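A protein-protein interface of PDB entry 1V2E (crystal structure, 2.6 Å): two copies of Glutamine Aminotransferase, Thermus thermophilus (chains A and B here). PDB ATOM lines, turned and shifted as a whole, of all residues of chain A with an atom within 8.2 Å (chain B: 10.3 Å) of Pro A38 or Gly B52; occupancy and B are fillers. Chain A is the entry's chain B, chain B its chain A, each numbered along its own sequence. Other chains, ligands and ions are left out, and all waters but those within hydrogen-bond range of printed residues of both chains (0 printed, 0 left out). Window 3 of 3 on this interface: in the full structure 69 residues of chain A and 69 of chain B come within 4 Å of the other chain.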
ATOM      1  N   PRO A  35       2.323  25.969  25.909  1.00  0.00           N
ATOM      2  CA  PRO A  35       1.785  26.114  24.552  1.00  0.00           C
ATOM      3  C   PRO A  35       0.277  26.292  24.489  1.00  0.00           C
ATOM      4  O   PRO A  35      -0.459  25.741  25.305  1.00  0.00           O
ATOM      5  CB  PRO A  35       2.230  24.824  23.863  1.00  0.00           C
ATOM      6  CG  PRO A  35       3.481  24.473  24.575  1.00  0.00           C
ATOM      7  CD  PRO A  35       3.130  24.743  26.015  1.00  0.00           C
ATOM      8  N   SER A  36      -0.175  27.056  23.503  1.00  0.00           N
ATOM      9  CA  SER A  36      -1.599  27.296  23.309  1.00  0.00           C
ATOM     10  C   SER A  36      -2.206  26.166  22.490  1.00  0.00           C
ATOM     11  O   SER A  36      -3.413  25.970  22.484  1.00  0.00           O
ATOM     12  CB  SER A  36      -1.823  28.631  22.583  1.00  0.00           C
ATOM     13  OG  SER A  36      -1.430  29.720  23.401  1.00  0.00           O
ATOM     14  N   ASN A  37      -1.359  25.429  21.788  1.00  0.00           N
ATOM     15  CA  ASN A  37      -1.824  24.324  20.965  1.00  0.00           C
ATOM     16  C   ASN A  37      -1.713  23.012  21.739  1.00  0.00           C
ATOM     17  O   ASN A  37      -1.093  22.955  22.806  1.00  0.00           O
ATOM     18  CB  ASN A  37      -0.990  24.248  19.690  1.00  0.00           C
ATOM     19  CG  ASN A  37       0.488  24.097  19.976  1.00  0.00           C
ATOM     20  OD1 ASN A  37       0.936  23.048  20.429  1.00  0.00           O
ATOM     21  ND2 ASN A  37       1.253  25.154  19.729  1.00  0.00           N
ATOM     22  N   PRO A  38      -2.335  21.944  21.224  1.00  0.00           N
ATOM     23  CA  PRO A  38      -2.280  20.644  21.891  1.00  0.00           C
ATOM     24  C   PRO A  38      -1.045  19.874  21.425  1.00  0.00           C
ATOM     25  O   PRO A  38      -0.469  20.196  20.388  1.00  0.00           O
ATOM     26  CB  PRO A  38      -3.585  19.994  21.454  1.00  0.00           C
ATOM     27  CG  PRO A  38      -3.714  20.477  20.061  1.00  0.00           C
ATOM     28  CD  PRO A  38      -3.370  21.943  20.176  1.00  0.00           C
ATOM     29  N   PRO A  39      -0.615  18.854  22.192  1.00  0.00           N
ATOM     30  CA  PRO A  39       0.564  18.095  21.778  1.00  0.00           C
ATOM     31  C   PRO A  39       0.407  17.461  20.402  1.00  0.00           C
ATOM     32  O   PRO A  39      -0.697  17.354  19.884  1.00  0.00           O
ATOM     33  CB  PRO A  39       0.745  17.083  22.910  1.00  0.00           C
ATOM     34  CG  PRO A  39      -0.582  17.042  23.593  1.00  0.00           C
ATOM     35  CD  PRO A  39      -1.089  18.419  23.517  1.00  0.00           C
ATOM     36  N   PRO A  40       1.524  17.055  19.778  1.00  0.00           N
ATOM     37  CA  PRO A  40       1.450  16.439  18.451  1.00  0.00           C
ATOM     38  C   PRO A  40       0.563  15.196  18.401  1.00  0.00           C
ATOM     39  O   PRO A  40       0.373  14.509  19.401  1.00  0.00           O
ATOM     40  CB  PRO A  40       2.916  16.145  18.124  1.00  0.00           C
ATOM     41  CG  PRO A  40       3.530  15.939  19.471  1.00  0.00           C
ATOM     42  CD  PRO A  40       2.901  17.018  20.303  1.00  0.00           C
ATOM     43  N   PRO A  41      -0.005  14.905  17.223  1.00  0.00           N
ATOM     44  CA  PRO A  41      -0.884  13.747  17.016  1.00  0.00           C
ATOM     45  C   PRO A  41      -0.282  12.388  17.374  1.00  0.00           C
ATOM     46  O   PRO A  41      -0.991  11.507  17.861  1.00  0.00           O
ATOM     47  CB  PRO A  41      -1.238  13.848  15.532  1.00  0.00           C
ATOM     48  CG  PRO A  41      -1.264  15.333  15.314  1.00  0.00           C
ATOM     49  CD  PRO A  41      -0.007  15.782  16.037  1.00  0.00           C
ATOM     50  N   LEU A  43       1.687  11.721  19.749  1.00  0.00           N
ATOM     51  CA  LEU A  43       1.799  11.551  21.194  1.00  0.00           C
ATOM     52  C   LEU A  43       0.436  11.222  21.788  1.00  0.00           C
ATOM     53  O   LEU A  43       0.345  10.436  22.715  1.00  0.00           O
ATOM     54  CB  LEU A  43       2.351  12.813  21.868  1.00  0.00           C
ATOM     55  CG  LEU A  43       2.456  12.760  23.399  1.00  0.00           C
ATOM     56  CD1 LEU A  43       3.380  11.630  23.803  1.00  0.00           C
ATOM     57  CD2 LEU A  43       2.967  14.092  23.946  1.00  0.00           C
ATOM     58  N   LEU A  44      -0.622  11.824  21.249  1.00  0.00           N
ATOM     59  CA  LEU A  44      -1.968  11.572  21.742  1.00  0.00           C
ATOM     60  C   LEU A  44      -2.393  10.174  21.321  1.00  0.00           C
ATOM     61  O   LEU A  44      -3.032   9.452  22.086  1.00  0.00           O
ATOM     62  CB  LEU A  44      -2.957  12.598  21.184  1.00  0.00           C
ATOM     63  CG  LEU A  44      -2.601  14.069  21.427  1.00  0.00           C
ATOM     64  CD1 LEU A  44      -3.616  14.940  20.714  1.00  0.00           C
ATOM     65  CD2 LEU A  44      -2.562  14.382  22.932  1.00  0.00           C
ATOM     66  N   ARG A  48      -3.407   7.065  23.898  1.00  0.00           N
ATOM     67  CA  ARG A  48      -4.686   6.388  23.689  1.00  0.00           C
ATOM     68  C   ARG A  48      -4.504   4.887  23.584  1.00  0.00           C
ATOM     69  O   ARG A  48      -5.321   4.132  24.089  1.00  0.00           O
ATOM     70  CB  ARG A  48      -5.358   6.882  22.404  1.00  0.00           C
ATOM     71  CG  ARG A  48      -6.117   8.186  22.525  1.00  0.00           C
ATOM     72  CD  ARG A  48      -6.320   8.760  21.136  1.00  0.00           C
ATOM     73  NE  ARG A  48      -6.765  10.150  21.151  1.00  0.00           N
ATOM     74  CZ  ARG A  48      -6.483  11.031  20.191  1.00  0.00           C
ATOM     75  NH1 ARG A  48      -5.748  10.670  19.144  1.00  0.00           N
ATOM     76  NH2 ARG A  48      -6.954  12.269  20.267  1.00  0.00           N
ATOM     77  N   LEU A 224       7.713  17.816  24.027  1.00  0.00           N
ATOM     78  CA  LEU A 224       6.487  17.511  23.284  1.00  0.00           C
ATOM     79  C   LEU A 224       5.212  18.344  23.462  1.00  0.00           C
ATOM     80  O   LEU A 224       4.118  17.855  23.192  1.00  0.00           O
ATOM     81  CB  LEU A 224       6.156  16.037  23.527  1.00  0.00           C
ATOM     82  CG  LEU A 224       7.313  15.118  23.150  1.00  0.00           C
ATOM     83  CD1 LEU A 224       7.102  13.752  23.732  1.00  0.00           C
ATOM     84  CD2 LEU A 224       7.447  15.075  21.642  1.00  0.00           C
ATOM     85  N   GLU A 225       5.342  19.587  23.909  1.00  0.00           N
ATOM     86  CA  GLU A 225       4.174  20.438  24.077  1.00  0.00           C
ATOM     87  C   GLU A 225       3.101  19.788  24.950  1.00  0.00           C
ATOM     88  O   GLU A 225       1.913  19.938  24.695  1.00  0.00           O
ATOM     89  CB  GLU A 225       3.598  20.745  22.704  1.00  0.00           C
ATOM     90  CG  GLU A 225       4.634  21.267  21.717  1.00  0.00           C
ATOM     91  CD  GLU A 225       4.770  22.787  21.740  1.00  0.00           C
ATOM     92  OE1 GLU A 225       4.017  23.464  21.008  1.00  0.00           O
ATOM     93  OE2 GLU A 225       5.623  23.301  22.497  1.00  0.00           O
ATOM     94  N   ALA A 226       3.520  19.065  25.983  1.00  0.00           N
ATOM     95  CA  ALA A 226       2.587  18.396  26.876  1.00  0.00           C
ATOM     96  C   ALA A 226       3.062  18.579  28.304  1.00  0.00           C
ATOM     97  O   ALA A 226       3.380  17.608  28.990  1.00  0.00           O
ATOM     98  CB  ALA A 226       2.521  16.920  26.541  1.00  0.00           C
ATOM     99  N   TYR A 229       1.758  16.450  31.440  1.00  0.00           N
ATOM    100  CA  TYR A 229       1.923  15.008  31.516  1.00  0.00           C
ATOM    101  C   TYR A 229       2.748  14.565  32.705  1.00  0.00           C
ATOM    102  O   TYR A 229       2.634  13.422  33.156  1.00  0.00           O
ATOM    103  CB  TYR A 229       2.494  14.464  30.204  1.00  0.00           C
ATOM    104  CG  TYR A 229       1.439  14.382  29.099  1.00  0.00           C
ATOM    105  CD1 TYR A 229       0.229  15.073  29.215  1.00  0.00           C
ATOM    106  CD2 TYR A 229       1.670  13.661  27.926  1.00  0.00           C
ATOM    107  CE1 TYR A 229      -0.711  15.053  28.198  1.00  0.00           C
ATOM    108  CE2 TYR A 229       0.730  13.638  26.900  1.00  0.00           C
ATOM    109  CZ  TYR A 229      -0.459  14.339  27.045  1.00  0.00           C
ATOM    110  OH  TYR A 229      -1.403  14.339  26.042  1.00  0.00           O
ATOM    111  N   PHE A 275      10.144  15.897  13.792  1.00  0.00           N
ATOM    112  CA  PHE A 275       9.315  16.772  14.603  1.00  0.00           C
ATOM    113  C   PHE A 275      10.066  17.956  15.234  1.00  0.00           C
ATOM    114  O   PHE A 275       9.686  19.111  15.035  1.00  0.00           O
ATOM    115  CB  PHE A 275       8.643  15.958  15.699  1.00  0.00           C
ATOM    116  CG  PHE A 275       7.839  16.784  16.654  1.00  0.00           C
ATOM    117  CD1 PHE A 275       6.651  17.368  16.250  1.00  0.00           C
ATOM    118  CD2 PHE A 275       8.278  16.977  17.967  1.00  0.00           C
ATOM    119  CE1 PHE A 275       5.902  18.135  17.137  1.00  0.00           C
ATOM    120  CE2 PHE A 275       7.535  17.743  18.861  1.00  0.00           C
ATOM    121  CZ  PHE A 275       6.343  18.323  18.448  1.00  0.00           C
ATOM    122  N   LEU A 279       9.663  21.936  15.005  1.00  0.00           N
ATOM    123  CA  LEU A 279       9.217  22.616  16.205  1.00  0.00           C
ATOM    124  C   LEU A 279      10.089  23.844  16.415  1.00  0.00           C
ATOM    125  O   LEU A 279       9.631  24.873  16.915  1.00  0.00           O
ATOM    126  CB  LEU A 279       9.296  21.698  17.428  1.00  0.00           C
ATOM    127  CG  LEU A 279       8.433  22.189  18.595  1.00  0.00           C
ATOM    128  CD1 LEU A 279       7.019  22.405  18.098  1.00  0.00           C
ATOM    129  CD2 LEU A 279       8.440  21.191  19.740  1.00  0.00           C
ATOM    130  N   ALA B  46     -13.433   9.044  30.048  1.00  0.00           N
ATOM    131  CA  ALA B  46     -13.291  10.390  30.577  1.00  0.00           C
ATOM    132  C   ALA B  46     -11.864  10.902  30.324  1.00  0.00           C
ATOM    133  O   ALA B  46     -11.655  12.083  30.054  1.00  0.00           O
ATOM    134  CB  ALA B  46     -13.612  10.395  32.042  1.00  0.00           C
ATOM    135  N   VAL B  47     -10.878  10.013  30.393  1.00  0.00           N
ATOM    136  CA  VAL B  47      -9.496  10.409  30.146  1.00  0.00           C
ATOM    137  C   VAL B  47      -9.282  10.690  28.661  1.00  0.00           C
ATOM    138  O   VAL B  47      -8.622  11.665  28.301  1.00  0.00           O
ATOM    139  CB  VAL B  47      -8.516   9.318  30.619  1.00  0.00           C
ATOM    140  CG1 VAL B  47      -7.134   9.570  30.074  1.00  0.00           C
ATOM    141  CG2 VAL B  47      -8.488   9.294  32.132  1.00  0.00           C
ATOM    142  N   ARG B  48      -9.841   9.832  27.806  1.00  0.00           N
ATOM    143  CA  ARG B  48      -9.747   9.985  26.348  1.00  0.00           C
ATOM    144  C   ARG B  48     -10.291  11.341  25.901  1.00  0.00           C
ATOM    145  O   ARG B  48      -9.750  12.003  25.026  1.00  0.00           O
ATOM    146  CB  ARG B  48     -10.571   8.903  25.647  1.00  0.00           C
ATOM    147  CG  ARG B  48      -9.768   7.767  25.086  1.00  0.00           C
ATOM    148  CD  ARG B  48     -10.354   7.289  23.779  1.00  0.00           C
ATOM    149  NE  ARG B  48      -9.475   6.304  23.158  1.00  0.00           N
ATOM    150  CZ  ARG B  48      -9.204   5.124  23.701  1.00  0.00           C
ATOM    151  NH1 ARG B  48      -9.755   4.791  24.862  1.00  0.00           N
ATOM    152  NH2 ARG B  48      -8.368   4.290  23.100  1.00  0.00           N
ATOM    153  N   ARG B  49     -11.395  11.719  26.515  1.00  0.00           N
ATOM    154  CA  ARG B  49     -12.088  12.958  26.237  1.00  0.00           C
ATOM    155  C   ARG B  49     -11.247  14.173  26.657  1.00  0.00           C
ATOM    156  O   ARG B  49     -11.419  15.273  26.129  1.00  0.00           O
ATOM    157  CB  ARG B  49     -13.393  12.900  27.006  1.00  0.00           C
ATOM    158  CG  ARG B  49     -14.449  13.890  26.676  1.00  0.00           C
ATOM    159  CD  ARG B  49     -15.664  13.483  27.485  1.00  0.00           C
ATOM    160  NE  ARG B  49     -16.000  12.081  27.214  1.00  0.00           N
ATOM    161  CZ  ARG B  49     -16.491  11.236  28.118  1.00  0.00           C
ATOM    162  NH1 ARG B  49     -16.701  11.638  29.371  1.00  0.00           N
ATOM    163  NH2 ARG B  49     -16.788   9.988  27.764  1.00  0.00           N
ATOM    164  N   ALA B  50     -10.324  13.969  27.593  1.00  0.00           N
ATOM    165  CA  ALA B  50      -9.474  15.049  28.072  1.00  0.00           C
ATOM    166  C   ALA B  50      -8.203  15.250  27.246  1.00  0.00           C
ATOM    167  O   ALA B  50      -7.634  16.346  27.222  1.00  0.00           O
ATOM    168  CB  ALA B  50      -9.113  14.805  29.524  1.00  0.00           C
ATOM    169  N   LEU B  51      -7.747  14.202  26.569  1.00  0.00           N
ATOM    170  CA  LEU B  51      -6.533  14.322  25.774  1.00  0.00           C
ATOM    171  C   LEU B  51      -6.726  15.238  24.582  1.00  0.00           C
ATOM    172  O   LEU B  51      -7.756  15.191  23.908  1.00  0.00           O
ATOM    173  CB  LEU B  51      -6.066  12.946  25.299  1.00  0.00           C
ATOM    174  CG  LEU B  51      -5.623  11.997  26.413  1.00  0.00           C
ATOM    175  CD1 LEU B  51      -5.441  10.631  25.815  1.00  0.00           C
ATOM    176  CD2 LEU B  51      -4.336  12.481  27.079  1.00  0.00           C
ATOM    177  N   GLY B  52      -5.724  16.072  24.326  1.00  0.00           N
ATOM    178  CA  GLY B  52      -5.793  16.994  23.213  1.00  0.00           C
ATOM    179  C   GLY B  52      -6.552  18.271  23.538  1.00  0.00           C
ATOM    180  O   GLY B  52      -6.789  19.088  22.649  1.00  0.00           O
ATOM    181  N   ARG B  53      -6.936  18.450  24.799  1.00  0.00           N
ATOM    182  CA  ARG B  53      -7.675  19.642  25.199  1.00  0.00           C
ATOM    183  C   ARG B  53      -7.406  20.090  26.626  1.00  0.00           C
ATOM    184  O   ARG B  53      -7.823  21.162  27.037  1.00  0.00           O
ATOM    185  CB  ARG B  53      -9.176  19.417  24.989  1.00  0.00           C
ATOM    186  CG  ARG B  53      -9.664  18.070  25.459  1.00  0.00           C
ATOM    187  CD  ARG B  53     -11.040  17.768  24.899  1.00  0.00           C
ATOM    188  NE  ARG B  53     -12.048  18.703  25.392  1.00  0.00           N
ATOM    189  CZ  ARG B  53     -12.400  18.836  26.670  1.00  0.00           C
ATOM    190  NH1 ARG B  53     -11.825  18.090  27.611  1.00  0.00           N
ATOM    191  NH2 ARG B  53     -13.331  19.722  27.006  1.00  0.00           N
ATOM    192  N   GLN B  54      -6.702  19.264  27.379  1.00  0.00           N
ATOM    193  CA  GLN B  54      -6.340  19.583  28.753  1.00  0.00           C
ATOM    194  C   GLN B  54      -5.029  18.872  29.024  1.00  0.00           C
ATOM    195  O   GLN B  54      -4.909  18.066  29.941  1.00  0.00           O
ATOM    196  CB  GLN B  54      -7.431  19.127  29.720  1.00  0.00           C
ATOM    197  CG  GLN B  54      -8.515  20.176  29.932  1.00  0.00           C
ATOM    198  CD  GLN B  54      -9.622  19.696  30.842  1.00  0.00           C
ATOM    199  OE1 GLN B  54     -10.456  18.872  30.443  1.00  0.00           O
ATOM    200  NE2 GLN B  54      -9.638  20.200  32.077  1.00  0.00           N
ATOM    201  N   ASP B  55      -4.043  19.205  28.200  1.00  0.00           N
ATOM    202  CA  ASP B  55      -2.718  18.611  28.261  1.00  0.00           C
ATOM    203  C   ASP B  55      -1.655  19.400  29.006  1.00  0.00           C
ATOM    204  O   ASP B  55      -0.632  18.834  29.402  1.00  0.00           O
ATOM    205  CB  ASP B  55      -2.232  18.366  26.837  1.00  0.00           C
ATOM    206  CG  ASP B  55      -3.244  17.613  26.011  1.00  0.00           C
ATOM    207  OD1 ASP B  55      -3.610  16.483  26.400  1.00  0.00           O
ATOM    208  OD2 ASP B  55      -3.681  18.150  24.976  1.00  0.00           O
ATOM    209  N   GLN B  56      -1.898  20.695  29.199  1.00  0.00           N
ATOM    210  CA  GLN B  56      -0.935  21.576  29.851  1.00  0.00           C
ATOM    211  C   GLN B  56      -1.109  21.672  31.352  1.00  0.00           C
ATOM    212  O   GLN B  56      -2.021  21.076  31.922  1.00  0.00           O
ATOM    213  CB  GLN B  56      -1.021  22.968  29.242  1.00  0.00           C
ATOM    214  CG  GLN B  56      -1.029  22.976  27.733  1.00  0.00           C
ATOM    215  CD  GLN B  56       0.207  22.320  27.151  1.00  0.00           C
ATOM    216  OE1 GLN B  56       1.264  22.275  27.799  1.00  0.00           O
ATOM    217  NE2 GLN B  56       0.093  21.825  25.914  1.00  0.00           N
ATOM    218  N   THR B 257      -2.622  16.514  34.124  1.00  0.00           N
ATOM    219  CA  THR B 257      -3.881  17.196  33.838  1.00  0.00           C
ATOM    220  C   THR B 257      -4.962  16.332  33.201  1.00  0.00           C
ATOM    221  O   THR B 257      -6.078  16.245  33.716  1.00  0.00           O
ATOM    222  CB  THR B 257      -3.623  18.439  32.984  1.00  0.00           C
ATOM    223  OG1 THR B 257      -2.564  19.192  33.582  1.00  0.00           O
ATOM    224  CG2 THR B 257      -4.848  19.311  32.929  1.00  0.00           C
ATOM    225  N   PRO B 258      -4.652  15.674  32.077  1.00  0.00           N
ATOM    226  CA  PRO B 258      -5.699  14.846  31.480  1.00  0.00           C
ATOM    227  C   PRO B 258      -6.186  13.765  32.449  1.00  0.00           C
ATOM    228  O   PRO B 258      -7.352  13.377  32.412  1.00  0.00           O
ATOM    229  CB  PRO B 258      -5.028  14.291  30.218  1.00  0.00           C
ATOM    230  CG  PRO B 258      -3.567  14.253  30.595  1.00  0.00           C
ATOM    231  CD  PRO B 258      -3.384  15.548  31.340  1.00  0.00           C
ATOM    232  N   LEU B 259      -5.313  13.288  33.330  1.00  0.00           N
ATOM    233  CA  LEU B 259      -5.741  12.276  34.287  1.00  0.00           C
ATOM    234  C   LEU B 259      -6.571  12.935  35.394  1.00  0.00           C
ATOM    235  O   LEU B 259      -7.515  12.347  35.928  1.00  0.00           O
ATOM    236  CB  LEU B 259      -4.534  11.551  34.865  1.00  0.00           C
ATOM    237  CG  LEU B 259      -3.957  10.400  34.035  1.00  0.00           C
ATOM    238  CD1 LEU B 259      -3.820  10.783  32.597  1.00  0.00           C
ATOM    239  CD2 LEU B 259      -2.613  10.007  34.609  1.00  0.00           C
ATOM    240  N   ALA B 261      -8.426  15.490  34.886  1.00  0.00           N
ATOM    241  CA  ALA B 261      -9.689  15.748  34.213  1.00  0.00           C
ATOM    242  C   ALA B 261     -10.577  14.493  34.231  1.00  0.00           C
ATOM    243  O   ALA B 261     -11.726  14.555  34.649  1.00  0.00           O
ATOM    244  CB  ALA B 261      -9.432  16.201  32.777  1.00  0.00           C
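Printed residues of chain A that touch a printed residue of chain B: Pro A35, Asn A37, Pro A38, Pro A39, Leu A44, Arg A48, Glu A225, Ala A226 and Tyr A229.
Hydrophobic or aromatic side chains of chain A within 4 Å of the printed part of chain B: Pro A35, Pro A38, Pro A39, Leu A44 and Tyr A229.
Of the 15 printed residues of chain B, 6 touch a printed residue of chain A.
Hydrophobic or aromatic side chains of chain B that line the printed part of chain A: Leu B51 and Pro B258.
Among the printed residues, 12 pairs touch across the chains.
Of the printed residues of chain B, Pro A35 touches Gln B56.
Asn A37 touches one residue of chain B.
Of chain B, only Gly B52 and Asp B55 come within 4 Å of Pro A38.
Pro A39 touches just one residue of chain B: Asp B55.
No residue of chain B comes within 4 Å of Pro A40.
Of the printed residues of chain B, Tyr A229 touches Leu B51 (3.6 Å), Asp B55 (3.1 Å) and Pro B258 (3.8 Å).
Ala B46 touches none of the printed residues of chain A.
Printed residues of chain A within 4 Å of Arg B48: Arg A48 (3.2 Å).
Ala B50 touches none of the printed residues of chain A.
Of the printed residues of chain A, Leu B51 touches Tyr A229 (3.6 Å).
Printed residues of chain A within 4 Å of Asp B55: Pro A38 (3.98 Å), Pro A39 (3.0 Å), Ala A226 (3.9 Å) and Tyr A229 (3.1 Å).
The nearest residue of chain A that does not touch Gly B52 is Pro A39 (4.9 Å).
The guanidinium group of Arg B48 is in hydrogen-bond range of the backbone carbonyl oxygen of Arg A48 (3.2 Å).
The side-chain hydroxyl (OH) of Tyr A229 is in hydrogen-bond range of the side-chain carboxylate (OD1) of Asp B55.
NE2 of Gln B56 is in hydrogen-bond range of O of Glu A225 (2.9 Å).
Arg A48 touches its own counterpart, Arg B48.
1 position is printed for both chains.
Of the 12 pairs that touch across the chains among the printed residues, 1 has its exchanged pair printed and touching as well.
CD of Pro A35 touches OE1 of Gln B56 (3.6 Å).
Asn A37 touches Gln B56.
Pro A38 touches Gly B52.
Pro A38 touches Asp B55.
Pro A39 touches Asp B55 (CD to OD2, 3.0 Å).
CD2 of Leu A44 touches N of Gly B52, at 3.8 Å.
Ala A226 touches Asp B55 (C to O, 3.9 Å).
Leu B51 touches Tyr A229.
CG of Pro B258 touches CE1 of Tyr A229, 3.8 Å away.
The side-chain amide oxygen of Asn A37 lies close to the side-chain carboxylate of Glu A225 (3.2 Å).
O of Gln B56 lies within hydrogen-bond range of OG1 of Thr B257.
OD2 of Asp B55 lies within hydrogen-bond range of N of Arg B53 (3.3 Å).
The backbone NH (N) of Gly B52 lies close to the side-chain carboxylate (OD2) of Asp B55 (3.0 Å).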
